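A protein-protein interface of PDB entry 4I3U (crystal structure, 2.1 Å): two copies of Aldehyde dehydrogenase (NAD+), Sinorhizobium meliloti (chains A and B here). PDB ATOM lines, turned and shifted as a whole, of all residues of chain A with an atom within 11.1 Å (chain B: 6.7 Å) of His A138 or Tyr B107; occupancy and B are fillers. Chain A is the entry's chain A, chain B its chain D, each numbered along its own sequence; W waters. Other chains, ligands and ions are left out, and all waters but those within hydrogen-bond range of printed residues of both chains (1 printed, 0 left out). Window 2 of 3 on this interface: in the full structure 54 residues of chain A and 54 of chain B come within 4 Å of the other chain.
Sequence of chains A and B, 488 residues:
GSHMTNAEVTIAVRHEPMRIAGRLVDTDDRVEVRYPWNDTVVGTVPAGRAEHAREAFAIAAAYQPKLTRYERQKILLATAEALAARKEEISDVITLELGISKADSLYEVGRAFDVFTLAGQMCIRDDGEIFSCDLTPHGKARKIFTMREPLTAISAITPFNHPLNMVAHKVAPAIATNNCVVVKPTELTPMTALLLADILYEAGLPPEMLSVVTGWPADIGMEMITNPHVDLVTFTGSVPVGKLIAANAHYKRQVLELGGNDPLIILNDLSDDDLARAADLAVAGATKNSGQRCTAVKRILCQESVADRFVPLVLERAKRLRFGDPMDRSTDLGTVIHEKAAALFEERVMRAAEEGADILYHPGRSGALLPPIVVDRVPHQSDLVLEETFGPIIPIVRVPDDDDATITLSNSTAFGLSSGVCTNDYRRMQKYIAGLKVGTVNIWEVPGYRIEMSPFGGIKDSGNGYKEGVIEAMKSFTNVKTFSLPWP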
ATOM      1  N   SER A 132     -14.978  -6.692  17.236  1.00  0.00           N
ATOM      2  CA  SER A 132     -13.915  -7.673  16.942  1.00  0.00           C
ATOM      3  C   SER A 132     -12.641  -7.183  17.585  1.00  0.00           C
ATOM      4  O   SER A 132     -12.426  -5.973  17.647  1.00  0.00           O
ATOM      5  CB  SER A 132     -13.701  -7.847  15.440  1.00  0.00           C
ATOM      6  OG  SER A 132     -14.813  -8.489  14.871  1.00  0.00           O
ATOM      7  N   CYS A 133     -11.791  -8.102  18.064  1.00  0.00           N
ATOM      8  CA  CYS A 133     -10.674  -7.690  18.921  1.00  0.00           C
ATOM      9  C   CYS A 133      -9.314  -7.770  18.250  1.00  0.00           C
ATOM     10  O   CYS A 133      -8.312  -7.412  18.857  1.00  0.00           O
ATOM     11  CB  CYS A 133     -10.670  -8.479  20.237  1.00  0.00           C
ATOM     12  SG  CYS A 133     -12.140  -8.109  21.187  1.00  0.00           S
ATOM     13  N   ASP A 134      -9.284  -8.226  16.999  1.00  0.00           N
ATOM     14  CA  ASP A 134      -8.022  -8.465  16.294  1.00  0.00           C
ATOM     15  C   ASP A 134      -7.634  -7.215  15.540  1.00  0.00           C
ATOM     16  O   ASP A 134      -7.408  -7.245  14.332  1.00  0.00           O
ATOM     17  CB  ASP A 134      -8.140  -9.651  15.332  1.00  0.00           C
ATOM     18  CG  ASP A 134      -9.298  -9.494  14.361  1.00  0.00           C
ATOM     19  OD1 ASP A 134     -10.395  -9.054  14.779  1.00  0.00           O
ATOM     20  OD2 ASP A 134      -9.140  -9.802  13.172  1.00  0.00           O
ATOM     21  N   LEU A 135      -7.540  -6.112  16.269  1.00  0.00           N
ATOM     22  CA  LEU A 135      -7.538  -4.793  15.654  1.00  0.00           C
ATOM     23  C   LEU A 135      -6.188  -4.090  15.599  1.00  0.00           C
ATOM     24  O   LEU A 135      -5.979  -3.247  14.754  1.00  0.00           O
ATOM     25  CB  LEU A 135      -8.511  -3.896  16.422  1.00  0.00           C
ATOM     26  CG  LEU A 135      -9.960  -3.846  15.941  1.00  0.00           C
ATOM     27  CD1 LEU A 135     -10.562  -5.212  15.656  1.00  0.00           C
ATOM     28  CD2 LEU A 135     -10.805  -3.060  16.933  1.00  0.00           C
ATOM     29  N   THR A 136      -5.297  -4.419  16.531  1.00  0.00           N
ATOM     30  CA  THR A 136      -4.012  -3.751  16.660  1.00  0.00           C
ATOM     31  C   THR A 136      -2.953  -4.835  16.893  1.00  0.00           C
ATOM     32  O   THR A 136      -3.290  -6.022  16.936  1.00  0.00           O
ATOM     33  CB  THR A 136      -4.022  -2.804  17.898  1.00  0.00           C
ATOM     34  OG1 THR A 136      -4.116  -3.575  19.113  1.00  0.00           O
ATOM     35  CG2 THR A 136      -5.181  -1.843  17.839  1.00  0.00           C
ATOM     36  N   PRO A 137      -1.681  -4.430  17.093  1.00  0.00           N
ATOM     37  CA  PRO A 137      -0.662  -5.395  17.541  1.00  0.00           C
ATOM     38  C   PRO A 137      -1.005  -6.085  18.854  1.00  0.00           C
ATOM     39  O   PRO A 137      -0.462  -7.162  19.110  1.00  0.00           O
ATOM     40  CB  PRO A 137       0.589  -4.534  17.721  1.00  0.00           C
ATOM     41  CG  PRO A 137       0.375  -3.387  16.757  1.00  0.00           C
ATOM     42  CD  PRO A 137      -1.098  -3.098  16.848  1.00  0.00           C
ATOM     43  N   HIS A 138      -1.884  -5.498  19.662  1.00  0.00           N
ATOM     44  CA  HIS A 138      -2.283  -6.139  20.916  1.00  0.00           C
ATOM     45  C   HIS A 138      -3.546  -6.953  20.729  1.00  0.00           C
ATOM     46  O   HIS A 138      -4.126  -7.395  21.712  1.00  0.00           O
ATOM     47  CB  HIS A 138      -2.514  -5.104  22.011  1.00  0.00           C
ATOM     48  CG  HIS A 138      -1.248  -4.580  22.613  1.00  0.00           C
ATOM     49  ND1 HIS A 138      -1.229  -3.555  23.539  1.00  0.00           N
ATOM     50  CD2 HIS A 138       0.048  -4.938  22.427  1.00  0.00           C
ATOM     51  CE1 HIS A 138       0.018  -3.310  23.901  1.00  0.00           C
ATOM     52  NE2 HIS A 138       0.813  -4.138  23.243  1.00  0.00           N
ATOM     53  N   GLY A 139      -3.955  -7.163  19.471  1.00  0.00           N
ATOM     54  CA  GLY A 139      -5.224  -7.818  19.143  1.00  0.00           C
ATOM     55  C   GLY A 139      -5.327  -9.280  19.539  1.00  0.00           C
ATOM     56  O   GLY A 139      -4.309  -9.934  19.770  1.00  0.00           O
ATOM     57  N   LYS A 140      -6.557  -9.784  19.611  1.00  0.00           N
ATOM     58  CA  LYS A 140      -6.792 -11.170  19.994  1.00  0.00           C
ATOM     59  C   LYS A 140      -7.948 -11.722  19.155  1.00  0.00           C
ATOM     60  O   LYS A 140      -8.760 -10.938  18.644  1.00  0.00           O
ATOM     61  CB  LYS A 140      -7.062 -11.267  21.491  1.00  0.00           C
ATOM     62  CG  LYS A 140      -5.778 -11.241  22.334  1.00  0.00           C
ATOM     63  CD  LYS A 140      -6.113 -11.046  23.799  1.00  0.00           C
ATOM     64  CE  LYS A 140      -4.954 -11.329  24.774  1.00  0.00           C
ATOM     65  NZ  LYS A 140      -3.614 -11.564  24.147  1.00  0.00           N
ATOM     66  N   ALA A 141      -7.982 -13.034  18.944  1.00  0.00           N
ATOM     67  CA  ALA A 141      -9.092 -13.684  18.235  1.00  0.00           C
ATOM     68  C   ALA A 141     -10.238 -13.844  19.197  1.00  0.00           C
ATOM     69  O   ALA A 141     -10.415 -14.919  19.802  1.00  0.00           O
ATOM     70  CB  ALA A 141      -8.657 -15.062  17.702  1.00  0.00           C
ATOM     71  N   ARG A 142     -11.035 -12.781  19.302  1.00  0.00           N
ATOM     72  CA  ARG A 142     -12.035 -12.662  20.362  1.00  0.00           C
ATOM     73  C   ARG A 142     -13.096 -11.643  19.936  1.00  0.00           C
ATOM     74  O   ARG A 142     -12.827 -10.749  19.126  1.00  0.00           O
ATOM     75  CB  ARG A 142     -11.329 -12.199  21.656  1.00  0.00           C
ATOM     76  CG  ARG A 142     -12.205 -11.830  22.837  1.00  0.00           C
ATOM     77  CD  ARG A 142     -11.303 -11.731  24.131  1.00  0.00           C
ATOM     78  NE  ARG A 142     -10.781 -13.036  24.483  1.00  0.00           N
ATOM     79  CZ  ARG A 142     -11.394 -13.860  25.311  1.00  0.00           C
ATOM     80  NH1 ARG A 142     -12.522 -13.478  25.873  1.00  0.00           N
ATOM     81  NH2 ARG A 142     -10.880 -15.037  25.563  1.00  0.00           N
ATOM     82  N   ILE A 144     -16.134  -8.978  21.620  1.00  0.00           N
ATOM     83  CA  ILE A 144     -16.780  -8.343  22.785  1.00  0.00           C
ATOM     84  C   ILE A 144     -18.221  -8.044  22.386  1.00  0.00           C
ATOM     85  O   ILE A 144     -18.474  -7.584  21.282  1.00  0.00           O
ATOM     86  CB  ILE A 144     -16.072  -7.061  23.158  1.00  0.00           C
ATOM     87  CG1 ILE A 144     -14.668  -7.384  23.708  1.00  0.00           C
ATOM     88  CG2 ILE A 144     -16.871  -6.238  24.181  1.00  0.00           C
ATOM     89  CD1 ILE A 144     -13.736  -6.145  23.799  1.00  0.00           C
ATOM     90  N   SER B  91       9.261   5.265  27.991  1.00  0.00           N
ATOM     91  CA  SER B  91       9.167   4.243  29.005  1.00  0.00           C
ATOM     92  C   SER B  91      10.247   4.402  30.085  1.00  0.00           C
ATOM     93  O   SER B  91      10.043   4.007  31.240  1.00  0.00           O
ATOM     94  CB  SER B  91       9.170   2.844  28.403  1.00  0.00           C
ATOM     95  OG  SER B  91      10.384   2.616  27.755  1.00  0.00           O
ATOM     96  N   SER B 101       8.578  -2.266  35.815  1.00  0.00           N
ATOM     97  CA  SER B 101       9.633  -2.727  34.894  1.00  0.00           C
ATOM     98  C   SER B 101       9.555  -2.058  33.519  1.00  0.00           C
ATOM     99  O   SER B 101       8.485  -1.646  33.071  1.00  0.00           O
ATOM    100  CB  SER B 101       9.557  -4.250  34.733  1.00  0.00           C
ATOM    101  OG  SER B 101       8.379  -4.632  34.023  1.00  0.00           O
ATOM    102  N   LYS B 102      10.695  -1.934  32.854  1.00  0.00           N
ATOM    103  CA  LYS B 102      10.710  -1.536  31.454  1.00  0.00           C
ATOM    104  C   LYS B 102       9.795  -2.408  30.553  1.00  0.00           C
ATOM    105  O   LYS B 102       9.179  -1.912  29.607  1.00  0.00           O
ATOM    106  CB  LYS B 102      12.135  -1.553  30.910  1.00  0.00           C
ATOM    107  CG  LYS B 102      12.967  -0.368  31.356  1.00  0.00           C
ATOM    108  CD  LYS B 102      12.684   0.862  30.510  1.00  0.00           C
ATOM    109  CE  LYS B 102      13.038   0.645  29.032  1.00  0.00           C
ATOM    110  NZ  LYS B 102      13.028   1.934  28.245  1.00  0.00           N
ATOM    111  N   ALA B 103       9.707  -3.697  30.836  1.00  0.00           N
ATOM    112  CA  ALA B 103       8.748  -4.543  30.119  1.00  0.00           C
ATOM    113  C   ALA B 103       7.323  -3.983  30.209  1.00  0.00           C
ATOM    114  O   ALA B 103       6.639  -3.808  29.190  1.00  0.00           O
ATOM    115  CB  ALA B 103       8.793  -5.984  30.649  1.00  0.00           C
ATOM    116  N   ASP B 104       6.862  -3.725  31.427  1.00  0.00           N
ATOM    117  CA  ASP B 104       5.541  -3.108  31.643  1.00  0.00           C
ATOM    118  C   ASP B 104       5.442  -1.692  31.062  1.00  0.00           C
ATOM    119  O   ASP B 104       4.434  -1.325  30.461  1.00  0.00           O
ATOM    120  CB  ASP B 104       5.175  -3.107  33.129  1.00  0.00           C
ATOM    121  CG  ASP B 104       4.810  -4.488  33.637  1.00  0.00           C
ATOM    122  OD1 ASP B 104       4.289  -5.302  32.844  1.00  0.00           O
ATOM    123  OD2 ASP B 104       5.033  -4.761  34.835  1.00  0.00           O
ATOM    124  N   SER B 105       6.486  -0.888  31.202  1.00  0.00           N
ATOM    125  CA  SER B 105       6.392   0.477  30.710  1.00  0.00           C
ATOM    126  C   SER B 105       6.483   0.563  29.197  1.00  0.00           C
ATOM    127  O   SER B 105       5.906   1.466  28.594  1.00  0.00           O
ATOM    128  CB  SER B 105       7.382   1.427  31.369  1.00  0.00           C
ATOM    129  OG  SER B 105       8.700   1.079  31.108  1.00  0.00           O
ATOM    130  N   LEU B 106       7.215  -0.356  28.575  1.00  0.00           N
ATOM    131  CA  LEU B 106       7.211  -0.426  27.117  1.00  0.00           C
ATOM    132  C   LEU B 106       5.830  -0.845  26.652  1.00  0.00           C
ATOM    133  O   LEU B 106       5.326  -0.351  25.643  1.00  0.00           O
ATOM    134  CB  LEU B 106       8.286  -1.394  26.599  1.00  0.00           C
ATOM    135  CG  LEU B 106       9.707  -0.831  26.628  1.00  0.00           C
ATOM    136  CD1 LEU B 106      10.750  -1.933  26.458  1.00  0.00           C
ATOM    137  CD2 LEU B 106       9.889   0.231  25.562  1.00  0.00           C
ATOM    138  N   TYR B 107       5.233  -1.779  27.377  1.00  0.00           N
ATOM    139  CA  TYR B 107       3.890  -2.214  27.038  1.00  0.00           C
ATOM    140  C   TYR B 107       2.911  -1.020  27.136  1.00  0.00           C
ATOM    141  O   TYR B 107       2.016  -0.854  26.289  1.00  0.00           O
ATOM    142  CB  TYR B 107       3.443  -3.367  27.938  1.00  0.00           C
ATOM    143  CG  TYR B 107       2.153  -4.001  27.466  1.00  0.00           C
ATOM    144  CD1 TYR B 107       2.171  -4.994  26.509  1.00  0.00           C
ATOM    145  CD2 TYR B 107       0.910  -3.559  27.933  1.00  0.00           C
ATOM    146  CE1 TYR B 107       0.992  -5.566  26.051  1.00  0.00           C
ATOM    147  CE2 TYR B 107      -0.276  -4.120  27.457  1.00  0.00           C
ATOM    148  CZ  TYR B 107      -0.224  -5.111  26.534  1.00  0.00           C
ATOM    149  OH  TYR B 107      -1.382  -5.688  26.072  1.00  0.00           O
ATOM    150  N   GLU B 108       3.094  -0.183  28.154  1.00  0.00           N
ATOM    151  CA  GLU B 108       2.207   0.964  28.333  1.00  0.00           C
ATOM    152  C   GLU B 108       2.281   1.890  27.119  1.00  0.00           C
ATOM    153  O   GLU B 108       1.265   2.430  26.666  1.00  0.00           O
ATOM    154  CB  GLU B 108       2.516   1.753  29.622  1.00  0.00           C
ATOM    155  CG  GLU B 108       1.489   2.865  29.868  1.00  0.00           C
ATOM    156  CD  GLU B 108       1.689   3.651  31.145  1.00  0.00           C
ATOM    157  OE1 GLU B 108       2.477   3.216  32.008  1.00  0.00           O
ATOM    158  OE2 GLU B 108       1.029   4.707  31.275  1.00  0.00           O
ATOM    159  N   VAL B 109       3.489   2.101  26.595  1.00  0.00           N
ATOM    160  CA  VAL B 109       3.621   2.959  25.432  1.00  0.00           C
ATOM    161  C   VAL B 109       2.871   2.356  24.246  1.00  0.00           C
ATOM    162  O   VAL B 109       2.253   3.071  23.464  1.00  0.00           O
ATOM    163  CB  VAL B 109       5.092   3.183  25.039  1.00  0.00           C
ATOM    164  CG1 VAL B 109       5.165   4.049  23.824  1.00  0.00           C
ATOM    165  CG2 VAL B 109       5.878   3.853  26.211  1.00  0.00           C
ATOM    166  N   GLY B 110       2.900   1.034  24.121  1.00  0.00           N
ATOM    167  CA  GLY B 110       2.073   0.362  23.130  1.00  0.00           C
ATOM    168  C   GLY B 110       0.574   0.626  23.297  1.00  0.00           C
ATOM    169  O   GLY B 110      -0.122   0.846  22.323  1.00  0.00           O
ATOM    170  N   ARG B 111       0.068   0.601  24.527  1.00  0.00           N
ATOM    171  CA  ARG B 111      -1.344   0.893  24.754  1.00  0.00           C
ATOM    172  C   ARG B 111      -1.621   2.333  24.318  1.00  0.00           C
ATOM    173  O   ARG B 111      -2.583   2.617  23.607  1.00  0.00           O
ATOM    174  CB  ARG B 111      -1.748   0.647  26.216  1.00  0.00           C
ATOM    175  CG  ARG B 111      -1.723  -0.852  26.624  1.00  0.00           C
ATOM    176  CD  ARG B 111      -2.408  -1.087  27.993  1.00  0.00           C
ATOM    177  NE  ARG B 111      -3.798  -0.657  27.954  1.00  0.00           N
ATOM    178  CZ  ARG B 111      -4.585  -0.512  29.019  1.00  0.00           C
ATOM    179  NH1 ARG B 111      -4.123  -0.771  30.251  1.00  0.00           N
ATOM    180  NH2 ARG B 111      -5.839  -0.096  28.843  1.00  0.00           N
ATOM    181  N   ALA B 112      -0.746   3.247  24.688  1.00  0.00           N
ATOM    182  CA  ALA B 112      -0.994   4.647  24.371  1.00  0.00           C
ATOM    183  C   ALA B 112      -0.951   4.848  22.849  1.00  0.00           C
ATOM    184  O   ALA B 112      -1.710   5.643  22.282  1.00  0.00           O
ATOM    185  CB  ALA B 112      -0.001   5.545  25.099  1.00  0.00           C
ATOM    186  N   ASP B 114      -1.980   2.595  20.776  1.00  0.00           N
ATOM    187  CA  ASP B 114      -3.316   2.170  20.340  1.00  0.00           C
ATOM    188  C   ASP B 114      -4.370   3.276  20.595  1.00  0.00           C
ATOM    189  O   ASP B 114      -5.202   3.550  19.741  1.00  0.00           O
ATOM    190  CB  ASP B 114      -3.748   0.910  21.090  1.00  0.00           C
ATOM    191  CG  ASP B 114      -3.130  -0.363  20.511  1.00  0.00           C
ATOM    192  OD1 ASP B 114      -2.330  -0.255  19.547  1.00  0.00           O
ATOM    193  OD2 ASP B 114      -3.478  -1.467  21.002  1.00  0.00           O
ATOM    194  N   LYS B 288       1.090  -8.271  36.362  1.00  0.00           N
ATOM    195  CA  LYS B 288       1.309  -7.190  35.380  1.00  0.00           C
ATOM    196  C   LYS B 288       1.234  -5.814  35.971  1.00  0.00           C
ATOM    197  O   LYS B 288       0.338  -5.558  36.765  1.00  0.00           O
ATOM    198  CB  LYS B 288       0.159  -7.148  34.398  1.00  0.00           C
ATOM    199  CG  LYS B 288       0.188  -7.996  33.295  1.00  0.00           C
ATOM    200  CD  LYS B 288       1.193  -7.914  32.286  1.00  0.00           C
ATOM    201  CE  LYS B 288       0.469  -7.420  31.018  1.00  0.00           C
ATOM    202  NZ  LYS B 288       1.365  -7.132  29.840  1.00  0.00           N
ATOM    203  N   ARG B 293      -3.379  -2.277  38.603  1.00  0.00           N
ATOM    204  CA  ARG B 293      -4.430  -2.009  37.619  1.00  0.00           C
ATOM    205  C   ARG B 293      -5.760  -2.080  38.322  1.00  0.00           C
ATOM    206  O   ARG B 293      -5.970  -2.964  39.154  1.00  0.00           O
ATOM    207  CB  ARG B 293      -4.417  -3.047  36.469  1.00  0.00           C
ATOM    208  CG  ARG B 293      -3.210  -2.952  35.534  1.00  0.00           C
ATOM    209  CD  ARG B 293      -3.349  -3.874  34.351  1.00  0.00           C
ATOM    210  NE  ARG B 293      -4.373  -3.389  33.421  1.00  0.00           N
ATOM    211  CZ  ARG B 293      -4.905  -4.123  32.442  1.00  0.00           C
ATOM    212  NH1 ARG B 293      -4.503  -5.381  32.290  1.00  0.00           N
ATOM    213  NH2 ARG B 293      -5.832  -3.628  31.622  1.00  0.00           N
ATOM    214  N   TYR B 449      -8.393  -7.469  30.312  1.00  0.00           N
ATOM    215  CA  TYR B 449      -8.457  -7.478  28.853  1.00  0.00           C
ATOM    216  C   TYR B 449      -9.595  -6.626  28.270  1.00  0.00           C
ATOM    217  O   TYR B 449     -10.765  -6.809  28.649  1.00  0.00           O
ATOM    218  CB  TYR B 449      -8.564  -8.909  28.239  1.00  0.00           C
ATOM    219  CG  TYR B 449      -8.603  -8.714  26.754  1.00  0.00           C
ATOM    220  CD1 TYR B 449      -7.427  -8.411  26.062  1.00  0.00           C
ATOM    221  CD2 TYR B 449      -9.817  -8.645  26.066  1.00  0.00           C
ATOM    222  CE1 TYR B 449      -7.456  -8.111  24.730  1.00  0.00           C
ATOM    223  CE2 TYR B 449      -9.841  -8.334  24.711  1.00  0.00           C
ATOM    224  CZ  TYR B 449      -8.658  -8.069  24.058  1.00  0.00           C
ATOM    225  OH  TYR B 449      -8.649  -7.768  22.717  1.00  0.00           O
ATOM    226  N   ARG B 450      -9.243  -5.761  27.311  1.00  0.00           N
ATOM    227  CA  ARG B 450     -10.207  -4.970  26.528  1.00  0.00           C
ATOM    228  C   ARG B 450      -9.442  -4.377  25.340  1.00  0.00           C
ATOM    229  O   ARG B 450      -8.221  -4.417  25.325  1.00  0.00           O
ATOM    230  CB  ARG B 450     -10.775  -3.831  27.380  1.00  0.00           C
ATOM    231  CG  ARG B 450      -9.706  -2.805  27.798  1.00  0.00           C
ATOM    232  CD  ARG B 450     -10.135  -1.874  28.951  1.00  0.00           C
ATOM    233  NE  ARG B 450     -10.012  -0.517  28.489  1.00  0.00           N
ATOM    234  CZ  ARG B 450      -9.677   0.534  29.220  1.00  0.00           C
ATOM    235  NH1 ARG B 450      -9.388   0.403  30.491  1.00  0.00           N
ATOM    236  NH2 ARG B 450      -9.618   1.732  28.658  1.00  0.00           N
ATOM    237  N   ILE B 451     -10.146  -3.819  24.359  1.00  0.00           N
ATOM    238  CA  ILE B 451      -9.495  -2.984  23.362  1.00  0.00           C
ATOM    239  C   ILE B 451      -9.653  -1.533  23.829  1.00  0.00           C
ATOM    240  O   ILE B 451     -10.525  -1.248  24.640  1.00  0.00           O
ATOM    241  CB  ILE B 451     -10.084  -3.165  21.948  1.00  0.00           C
ATOM    242  CG1 ILE B 451     -11.578  -2.939  21.955  1.00  0.00           C
ATOM    243  CG2 ILE B 451      -9.793  -4.569  21.402  1.00  0.00           C
ATOM    244  CD1 ILE B 451     -12.242  -3.307  20.647  1.00  0.00           C
ATOM    245  N   GLU B 452      -8.831  -0.620  23.319  1.00  0.00           N
ATOM    246  CA  GLU B 452      -8.765   0.707  23.925  1.00  0.00           C
ATOM    247  C   GLU B 452     -10.011   1.503  23.564  1.00  0.00           C
ATOM    248  O   GLU B 452     -10.231   2.598  24.081  1.00  0.00           O
ATOM    249  CB  GLU B 452      -7.466   1.447  23.550  1.00  0.00           C
ATOM    250  CG  GLU B 452      -6.161   0.634  23.837  1.00  0.00           C
ATOM    251  CD  GLU B 452      -5.816   0.437  25.329  1.00  0.00           C
ATOM    252  OE1 GLU B 452      -6.387   1.115  26.222  1.00  0.00           O
ATOM    253  OE2 GLU B 452      -4.949  -0.427  25.607  1.00  0.00           O
HETATM  254  O   HOH W   1      -6.699  -5.874  22.132  1.00  0.00           O
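No position is printed for both chains.
Of the 8 pairs that touch across the chains among the printed residues, none has its exchanged pair printed and touching as well.
O of Lys A140 sits at hydrogen-bond distance from N of Asp A134.
N of Cys A133 sits at hydrogen-bond distance from O of Arg A142 (3.0 Å).
The backbone carbonyl oxygen (O) of Cys A133 is in hydrogen-bond range of the backbone NH (N) of Lys A140 (3.0 Å).
The side-chain carboxylate of Glu B452 lies within salt-bridge range of the guanidinium group of Arg B111 (2.6 Å).
The side-chain hydroxyl (OG1) of Thr A136 lies within hydrogen-bond range of the backbone NH (N) of His A138 (3.0 Å).
Printed residues of chain A that touch a printed residue of chain B: Cys A133, Leu A135, Thr A136, His A138, Lys A140 and Arg A142.
Printed residues of chain B that touch a printed residue of chain A: Tyr B107, Arg B111, Asp B114, Tyr B449 and Ile B451.
Hydrophobic or aromatic side chains of chain B within 4 Å of the printed part of chain A: Tyr B107, Tyr B449 and Ile B451.
Among the printed residues, 8 pairs touch across the chains.
Among the printed residues, no Asp or Glu carboxylate lies within 4 Å of a Lys or Arg side-chain nitrogen of the other chain.
Among the printed residues, pairs that only touch across the chains: Cys A133 with Tyr B449 (3.3 Å), Lys A140 with Tyr B449 (3.4 Å), Arg A142 with Tyr B449 (3.7 Å), His A138 with Asp B114 (3.9 Å), His A138 with Arg B111 (3.96 Å) and Leu A135 with Ile B451 (3.99 Å).
Of chain A, only His A138 comes within 4 Å of Tyr B107.
No residue of chain A comes within 4 Å of Ala B103.
No residue of chain A comes within 4 Å of Ser B105.
Leu B106 touches none of the printed residues of chain A.
No residue of chain A comes within 4 Å of Val B109.
No residue of chain A comes within 4 Å of Gly B110.
Of chain A, only His A138 (3.96 Å) comes within 4 Å of Arg B111.
Printed residues of chain B within 4 Å of Thr A136: Asp B114.
Of the printed residues of chain A, Asp B114 touches Thr A136 (2.9 Å) and His A138 (3.9 Å).
Of the printed residues of chain B, Arg A142 touches Tyr B449 (3.7 Å).
The nearest printed residue of chain B that does not touch Thr A136 is Ile B451 (6.2 Å).
Water W1 bridges OH of Tyr B449 and O of His A138.
The side-chain hydroxyl (OH) of Tyr B107 lies within hydrogen-bond range of a ring nitrogen (ND1) of His A138 (3.3 Å).
The side-chain hydroxyl of Thr A136 is in hydrogen-bond range of the side-chain carboxylate of Asp B114 (2.9 Å).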
